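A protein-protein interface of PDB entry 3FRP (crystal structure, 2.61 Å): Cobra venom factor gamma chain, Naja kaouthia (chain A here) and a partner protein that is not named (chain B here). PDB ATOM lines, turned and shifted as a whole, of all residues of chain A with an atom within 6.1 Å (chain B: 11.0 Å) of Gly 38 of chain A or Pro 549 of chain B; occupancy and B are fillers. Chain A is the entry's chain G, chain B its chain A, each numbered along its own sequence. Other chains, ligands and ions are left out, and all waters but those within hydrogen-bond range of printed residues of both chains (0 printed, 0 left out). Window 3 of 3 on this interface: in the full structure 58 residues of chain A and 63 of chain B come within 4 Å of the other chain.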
ATOM      1  N   LEU A  30     -15.545  -1.559  -8.944  1.00  0.00           N
ATOM      2  CA  LEU A  30     -15.429  -2.777  -8.162  1.00  0.00           C
ATOM      3  C   LEU A  30     -15.950  -3.954  -8.982  1.00  0.00           C
ATOM      4  O   LEU A  30     -17.065  -4.439  -8.776  1.00  0.00           O
ATOM      5  CB  LEU A  30     -16.168  -2.648  -6.834  1.00  0.00           C
ATOM      6  CG  LEU A  30     -15.818  -1.498  -5.890  1.00  0.00           C
ATOM      7  CD1 LEU A  30     -16.333  -1.845  -4.522  1.00  0.00           C
ATOM      8  CD2 LEU A  30     -14.323  -1.197  -5.803  1.00  0.00           C
ATOM      9  N   GLU A  32     -14.627  -6.862  -9.075  1.00  0.00           N
ATOM     10  CA  GLU A  32     -14.362  -8.086  -8.325  1.00  0.00           C
ATOM     11  C   GLU A  32     -15.678  -8.735  -7.885  1.00  0.00           C
ATOM     12  O   GLU A  32     -16.736  -8.089  -7.935  1.00  0.00           O
ATOM     13  CB  GLU A  32     -13.479  -7.786  -7.105  1.00  0.00           C
ATOM     14  CG  GLU A  32     -12.037  -7.349  -7.439  1.00  0.00           C
ATOM     15  CD  GLU A  32     -11.890  -5.860  -7.804  1.00  0.00           C
ATOM     16  OE1 GLU A  32     -12.836  -5.064  -7.601  1.00  0.00           O
ATOM     17  OE2 GLU A  32     -10.808  -5.475  -8.299  1.00  0.00           O
ATOM     18  N   GLU A  33     -15.618 -10.005  -7.473  1.00  0.00           N
ATOM     19  CA  GLU A  33     -16.820 -10.727  -7.056  1.00  0.00           C
ATOM     20  C   GLU A  33     -17.070 -10.613  -5.556  1.00  0.00           C
ATOM     21  O   GLU A  33     -16.124 -10.602  -4.782  1.00  0.00           O
ATOM     22  CB  GLU A  33     -16.791 -12.187  -7.516  1.00  0.00           C
ATOM     23  CG  GLU A  33     -17.439 -12.386  -8.897  1.00  0.00           C
ATOM     24  CD  GLU A  33     -18.734 -13.203  -8.873  1.00  0.00           C
ATOM     25  OE1 GLU A  33     -18.699 -14.342  -8.346  1.00  0.00           O
ATOM     26  OE2 GLU A  33     -19.774 -12.730  -9.409  1.00  0.00           O
ATOM     27  N   PRO A  34     -18.352 -10.497  -5.157  1.00  0.00           N
ATOM     28  CA  PRO A  34     -18.787 -10.364  -3.759  1.00  0.00           C
ATOM     29  C   PRO A  34     -18.616 -11.653  -2.966  1.00  0.00           C
ATOM     30  O   PRO A  34     -18.653 -12.742  -3.546  1.00  0.00           O
ATOM     31  CB  PRO A  34     -20.279 -10.069  -3.894  1.00  0.00           C
ATOM     32  CG  PRO A  34     -20.660 -10.713  -5.199  1.00  0.00           C
ATOM     33  CD  PRO A  34     -19.495 -10.449  -6.087  1.00  0.00           C
ATOM     34  N   ASN A  35     -18.458 -11.514  -1.652  1.00  0.00           N
ATOM     35  CA  ASN A  35     -18.268 -12.637  -0.741  1.00  0.00           C
ATOM     36  C   ASN A  35     -19.609 -13.208  -0.289  1.00  0.00           C
ATOM     37  O   ASN A  35     -20.618 -13.063  -0.997  1.00  0.00           O
ATOM     38  CB  ASN A  35     -17.415 -12.203   0.474  1.00  0.00           C
ATOM     39  CG  ASN A  35     -17.839 -10.846   1.057  1.00  0.00           C
ATOM     40  OD1 ASN A  35     -18.916 -10.326   0.756  1.00  0.00           O
ATOM     41  ND2 ASN A  35     -16.980 -10.271   1.897  1.00  0.00           N
ATOM     42  N   SER A  36     -19.625 -13.857   0.879  1.00  0.00           N
ATOM     43  CA  SER A  36     -20.880 -14.262   1.512  1.00  0.00           C
ATOM     44  C   SER A  36     -21.728 -13.029   1.737  1.00  0.00           C
ATOM     45  O   SER A  36     -22.930 -13.017   1.460  1.00  0.00           O
ATOM     46  CB  SER A  36     -20.618 -14.913   2.866  1.00  0.00           C
ATOM     47  OG  SER A  36     -19.661 -15.951   2.749  1.00  0.00           O
ATOM     48  N   GLN A  37     -21.068 -11.981   2.223  1.00  0.00           N
ATOM     49  CA  GLN A  37     -21.728 -10.750   2.661  1.00  0.00           C
ATOM     50  C   GLN A  37     -22.331  -9.911   1.519  1.00  0.00           C
ATOM     51  O   GLN A  37     -23.026  -8.923   1.766  1.00  0.00           O
ATOM     52  CB  GLN A  37     -20.743  -9.913   3.498  1.00  0.00           C
ATOM     53  CG  GLN A  37     -20.046 -10.713   4.612  1.00  0.00           C
ATOM     54  CD  GLN A  37     -21.043 -11.399   5.553  1.00  0.00           C
ATOM     55  OE1 GLN A  37     -21.185 -12.630   5.545  1.00  0.00           O
ATOM     56  NE2 GLN A  37     -21.751 -10.599   6.352  1.00  0.00           N
ATOM     57  N   GLY A  38     -22.072 -10.315   0.276  1.00  0.00           N
ATOM     58  CA  GLY A  38     -22.416  -9.496  -0.888  1.00  0.00           C
ATOM     59  C   GLY A  38     -21.519  -8.279  -1.090  1.00  0.00           C
ATOM     60  O   GLY A  38     -21.909  -7.347  -1.793  1.00  0.00           O
ATOM     61  N   ILE A  39     -20.313  -8.303  -0.502  1.00  0.00           N
ATOM     62  CA  ILE A  39     -19.364  -7.171  -0.533  1.00  0.00           C
ATOM     63  C   ILE A  39     -18.118  -7.419  -1.413  1.00  0.00           C
ATOM     64  O   ILE A  39     -17.399  -8.403  -1.234  1.00  0.00           O
ATOM     65  CB  ILE A  39     -18.936  -6.757   0.905  1.00  0.00           C
ATOM     66  CG1 ILE A  39     -20.105  -6.085   1.628  1.00  0.00           C
ATOM     67  CG2 ILE A  39     -17.731  -5.818   0.881  1.00  0.00           C
ATOM     68  CD1 ILE A  39     -19.915  -5.908   3.133  1.00  0.00           C
ATOM     69  N   SER A  40     -17.864  -6.499  -2.344  1.00  0.00           N
ATOM     70  CA  SER A  40     -16.728  -6.598  -3.259  1.00  0.00           C
ATOM     71  C   SER A  40     -15.537  -5.776  -2.795  1.00  0.00           C
ATOM     72  O   SER A  40     -15.697  -4.701  -2.214  1.00  0.00           O
ATOM     73  CB  SER A  40     -17.136  -6.177  -4.661  1.00  0.00           C
ATOM     74  OG  SER A  40     -17.991  -7.153  -5.218  1.00  0.00           O
ATOM     75  N   THR A  63     -23.846   3.356  -7.328  1.00  0.00           N
ATOM     76  CA  THR A  63     -24.246   2.005  -7.746  1.00  0.00           C
ATOM     77  C   THR A  63     -25.663   2.084  -8.299  1.00  0.00           C
ATOM     78  O   THR A  63     -26.539   2.601  -7.616  1.00  0.00           O
ATOM     79  CB  THR A  63     -24.239   0.998  -6.551  1.00  0.00           C
ATOM     80  OG1 THR A  63     -23.006   1.096  -5.821  1.00  0.00           O
ATOM     81  CG2 THR A  63     -24.427  -0.428  -7.027  1.00  0.00           C
ATOM     82  N   LYS A  66     -28.384   1.411  -5.757  1.00  0.00           N
ATOM     83  CA  LYS A  66     -28.078   1.719  -4.370  1.00  0.00           C
ATOM     84  C   LYS A  66     -27.669   3.164  -4.202  1.00  0.00           C
ATOM     85  O   LYS A  66     -27.244   3.559  -3.125  1.00  0.00           O
ATOM     86  CB  LYS A  66     -27.016   0.766  -3.819  1.00  0.00           C
ATOM     87  CG  LYS A  66     -27.494  -0.690  -3.676  1.00  0.00           C
ATOM     88  CD  LYS A  66     -26.434  -1.555  -2.994  1.00  0.00           C
ATOM     89  CE  LYS A  66     -27.047  -2.686  -2.132  1.00  0.00           C
ATOM     90  NZ  LYS A  66     -27.337  -3.960  -2.872  1.00  0.00           N
ATOM     91  N   MET B 523     -27.380   3.825   1.129  1.00  0.00           N
ATOM     92  CA  MET B 523     -28.268   2.768   0.709  1.00  0.00           C
ATOM     93  C   MET B 523     -27.492   1.456   0.633  1.00  0.00           C
ATOM     94  O   MET B 523     -27.965   0.421   1.086  1.00  0.00           O
ATOM     95  CB  MET B 523     -28.879   3.119  -0.629  1.00  0.00           C
ATOM     96  CG  MET B 523     -30.284   2.671  -0.762  1.00  0.00           C
ATOM     97  SD  MET B 523     -31.023   3.489  -2.162  1.00  0.00           S
ATOM     98  CE  MET B 523     -30.830   5.176  -1.645  1.00  0.00           C
ATOM     99  N   GLY B 524     -26.301   1.522   0.036  1.00  0.00           N
ATOM    100  CA  GLY B 524     -25.345   0.417   0.051  1.00  0.00           C
ATOM    101  C   GLY B 524     -24.243   0.600   1.088  1.00  0.00           C
ATOM    102  O   GLY B 524     -24.507   0.971   2.229  1.00  0.00           O
ATOM    103  N   THR B 525     -23.003   0.356   0.670  1.00  0.00           N
ATOM    104  CA  THR B 525     -21.849   0.275   1.561  1.00  0.00           C
ATOM    105  C   THR B 525     -20.595   0.766   0.863  1.00  0.00           C
ATOM    106  O   THR B 525     -20.346   0.437  -0.295  1.00  0.00           O
ATOM    107  CB  THR B 525     -21.642  -1.173   2.047  1.00  0.00           C
ATOM    108  OG1 THR B 525     -22.818  -1.591   2.738  1.00  0.00           O
ATOM    109  CG2 THR B 525     -20.453  -1.302   2.988  1.00  0.00           C
ATOM    110  N   LEU B 526     -19.809   1.556   1.587  1.00  0.00           N
ATOM    111  CA  LEU B 526     -18.499   1.972   1.123  1.00  0.00           C
ATOM    112  C   LEU B 526     -17.565   2.253   2.301  1.00  0.00           C
ATOM    113  O   LEU B 526     -17.810   3.149   3.101  1.00  0.00           O
ATOM    114  CB  LEU B 526     -18.610   3.182   0.184  1.00  0.00           C
ATOM    115  CG  LEU B 526     -17.398   3.465  -0.696  1.00  0.00           C
ATOM    116  CD1 LEU B 526     -17.501   2.633  -1.928  1.00  0.00           C
ATOM    117  CD2 LEU B 526     -17.350   4.912  -1.069  1.00  0.00           C
ATOM    118  N   LEU B 545     -10.745  -1.162  -0.699  1.00  0.00           N
ATOM    119  CA  LEU B 545     -12.046  -0.579  -0.962  1.00  0.00           C
ATOM    120  C   LEU B 545     -13.079  -1.674  -0.911  1.00  0.00           C
ATOM    121  O   LEU B 545     -13.033  -2.624  -1.713  1.00  0.00           O
ATOM    122  CB  LEU B 545     -12.076   0.042  -2.347  1.00  0.00           C
ATOM    123  CG  LEU B 545     -11.226   1.277  -2.602  1.00  0.00           C
ATOM    124  CD1 LEU B 545     -11.511   1.735  -4.002  1.00  0.00           C
ATOM    125  CD2 LEU B 545     -11.537   2.385  -1.610  1.00  0.00           C
ATOM    126  N   GLU B 546     -13.995  -1.549   0.043  1.00  0.00           N
ATOM    127  CA  GLU B 546     -15.084  -2.488   0.181  1.00  0.00           C
ATOM    128  C   GLU B 546     -16.371  -1.778  -0.200  1.00  0.00           C
ATOM    129  O   GLU B 546     -16.740  -0.759   0.389  1.00  0.00           O
ATOM    130  CB  GLU B 546     -15.139  -3.036   1.605  1.00  0.00           C
ATOM    131  CG  GLU B 546     -14.000  -4.017   1.916  1.00  0.00           C
ATOM    132  CD  GLU B 546     -13.813  -4.294   3.401  1.00  0.00           C
ATOM    133  OE1 GLU B 546     -13.942  -3.358   4.221  1.00  0.00           O
ATOM    134  OE2 GLU B 546     -13.523  -5.458   3.751  1.00  0.00           O
ATOM    135  N   GLY B 547     -17.048  -2.308  -1.203  1.00  0.00           N
ATOM    136  CA  GLY B 547     -18.248  -1.672  -1.710  1.00  0.00           C
ATOM    137  C   GLY B 547     -19.146  -2.693  -2.352  1.00  0.00           C
ATOM    138  O   GLY B 547     -18.975  -3.902  -2.134  1.00  0.00           O
ATOM    139  N   ASP B 548     -20.104  -2.200  -3.135  1.00  0.00           N
ATOM    140  CA  ASP B 548     -21.130  -3.041  -3.751  1.00  0.00           C
ATOM    141  C   ASP B 548     -20.630  -3.511  -5.109  1.00  0.00           C
ATOM    142  O   ASP B 548     -19.881  -2.791  -5.765  1.00  0.00           O
ATOM    143  CB  ASP B 548     -22.456  -2.279  -3.899  1.00  0.00           C
ATOM    144  CG  ASP B 548     -22.981  -1.728  -2.566  1.00  0.00           C
ATOM    145  OD1 ASP B 548     -23.341  -2.535  -1.681  1.00  0.00           O
ATOM    146  OD2 ASP B 548     -23.063  -0.479  -2.413  1.00  0.00           O
ATOM    147  N   PRO B 549     -21.025  -4.727  -5.533  1.00  0.00           N
ATOM    148  CA  PRO B 549     -20.493  -5.200  -6.808  1.00  0.00           C
ATOM    149  C   PRO B 549     -20.938  -4.285  -7.946  1.00  0.00           C
ATOM    150  O   PRO B 549     -22.106  -3.909  -8.029  1.00  0.00           O
ATOM    151  CB  PRO B 549     -21.095  -6.605  -6.948  1.00  0.00           C
ATOM    152  CG  PRO B 549     -22.272  -6.632  -5.993  1.00  0.00           C
ATOM    153  CD  PRO B 549     -21.882  -5.733  -4.876  1.00  0.00           C
ATOM    154  N   GLY B 550     -19.991  -3.894  -8.785  1.00  0.00           N
ATOM    155  CA  GLY B 550     -20.278  -3.024  -9.906  1.00  0.00           C
ATOM    156  C   GLY B 550     -20.318  -1.545  -9.590  1.00  0.00           C
ATOM    157  O   GLY B 550     -20.850  -0.764 -10.384  1.00  0.00           O
ATOM    158  N   ALA B 551     -19.759  -1.144  -8.447  1.00  0.00           N
ATOM    159  CA  ALA B 551     -19.786   0.273  -8.055  1.00  0.00           C
ATOM    160  C   ALA B 551     -18.692   1.145  -8.715  1.00  0.00           C
ATOM    161  O   ALA B 551     -17.550   0.731  -8.838  1.00  0.00           O
ATOM    162  CB  ALA B 551     -19.754   0.408  -6.536  1.00  0.00           C
ATOM    163  N   ARG B 552     -19.053   2.350  -9.148  1.00  0.00           N
ATOM    164  CA  ARG B 552     -18.041   3.323  -9.535  1.00  0.00           C
ATOM    165  C   ARG B 552     -17.730   4.191  -8.334  1.00  0.00           C
ATOM    166  O   ARG B 552     -18.588   4.929  -7.840  1.00  0.00           O
ATOM    167  CB  ARG B 552     -18.476   4.170 -10.717  1.00  0.00           C
ATOM    168  CG  ARG B 552     -18.675   3.392 -11.994  1.00  0.00           C
ATOM    169  CD  ARG B 552     -19.105   4.317 -13.131  1.00  0.00           C
ATOM    170  NE  ARG B 552     -17.969   5.049 -13.701  1.00  0.00           N
ATOM    171  CZ  ARG B 552     -17.317   4.675 -14.803  1.00  0.00           C
ATOM    172  NH1 ARG B 552     -17.694   3.580 -15.462  1.00  0.00           N
ATOM    173  NH2 ARG B 552     -16.289   5.396 -15.253  1.00  0.00           N
ATOM    174  N   VAL B 553     -16.489   4.067  -7.875  1.00  0.00           N
ATOM    175  CA  VAL B 553     -15.986   4.734  -6.696  1.00  0.00           C
ATOM    176  C   VAL B 553     -15.035   5.863  -7.113  1.00  0.00           C
ATOM    177  O   VAL B 553     -14.132   5.664  -7.940  1.00  0.00           O
ATOM    178  CB  VAL B 553     -15.228   3.711  -5.825  1.00  0.00           C
ATOM    179  CG1 VAL B 553     -14.626   4.366  -4.552  1.00  0.00           C
ATOM    180  CG2 VAL B 553     -16.151   2.534  -5.474  1.00  0.00           C
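O of Ala 551 of chain B lies within hydrogen-bond range of N of Leu 30 of chain A, 3.0 Å away. The backbone carbonyl oxygen of Gly 547 of chain B lies within hydrogen-bond range of the backbone NH of Ser 40 of chain A (2.8 Å). The backbone carbonyl oxygen (O) of Leu 30 of chain A sits at hydrogen-bond distance from the backbone NH (N) of Gly 550 of chain B (3.0 Å). The backbone carbonyl oxygen (O) of Ser 40 of chain A sits close to the backbone carbonyl oxygen (O) of Leu 545 of chain B (3.4 Å).
The side-chain amide oxygen of Asn 35 of chain A sits at hydrogen-bond distance from the backbone NH of Gly 38 of chain A (3.2 Å). The side-chain amide oxygen of Asn 35 of chain A sits at hydrogen-bond distance from the backbone NH of Ile 39 of chain A (2.8 Å). The side-chain carboxylate (OD2) of Asp 548 of chain B sits at hydrogen-bond distance from the backbone NH (N) of Thr 525 of chain B (3.2 Å). The backbone carbonyl oxygen (O) of Glu 32 of chain A is in hydrogen-bond range of the side-chain hydroxyl (OG) of Ser 40 of chain A (3.1 Å).
Leu 30 of chain A touches Gly 547 of chain B (CD1 to CA, 3.4 Å). Leu 30 of chain A touches Asp 548 of chain B (CB to O, 3.9 Å). Pro 549 of chain B touches Leu 30 of chain A. Gly 38 of chain A touches Pro 549 of chain B. CB of Glu 546 of chain B touches CG2 of Ile 39 of chain A, 3.9 Å away. Gly 547 of chain B touches Ile 39 of chain A. O of Ser 40 of chain A touches CA of Glu 546 of chain B (3.3 Å). CA of Pro 549 of chain B touches OG of Ser 40 of chain A, 3.5 Å away. O of Lys 66 of chain A touches CB of Met 523 of chain B (3.0 Å). CD of Lys 66 of chain A touches CG of Asp 548 of chain B, 3.5 Å away.
No residue of chain B comes within 4 Å of Asn 35 of chain A. No residue of chain B comes within 4 Å of Gln 37 of chain A. Gly 38 of chain A touches just one residue of chain B: Pro 549. Of chain B, only Glu 546 and Gly 547 come within 4 Å of Ile 39 of chain A. Of chain B, only Leu 545, Glu 546, Gly 547 and Pro 549 come within 4 Å of Ser 40 of chain A. Of the printed residues of chain A, Met 523 of chain B touches Lys 66. Thr 525 of chain B touches none of the printed residues of chain A. Printed residues of chain A within 4 Å of Leu 545 of chain B: Ser 40. Of the printed residues of chain A, Glu 546 of chain B touches Ile 39 and Ser 40. Of the printed residues of chain A, Gly 547 of chain B touches Leu 30 (3.4 Å), Ile 39 (3.7 Å) and Ser 40 (2.8 Å). Of chain A, only Leu 30, Gly 38 and Ser 40 come within 4 Å of Pro 549 of chain B. Val 553 of chain B touches none of the printed residues of chain A. The nearest residue of chain B that does not touch Gly 38 of chain A is Gly 547 of chain B (4.5 Å). The nearest residue of chain A that does not touch Pro 549 of chain B is Pro 34 of chain A (4.3 Å).
Of the 12 printed residues of chain A, 6 touch a printed residue of chain B. Printed residues of chain A that touch a printed residue of chain B: Leu 30, Gly 38, Ile 39, Ser 40, Thr 63 and Lys 66. Among the printed residues, 17 pairs touch across the chains. Among the printed residues, no Asp or Glu carboxylate lies within 4 Å of a Lys or Arg side-chain nitrogen of the other chain.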
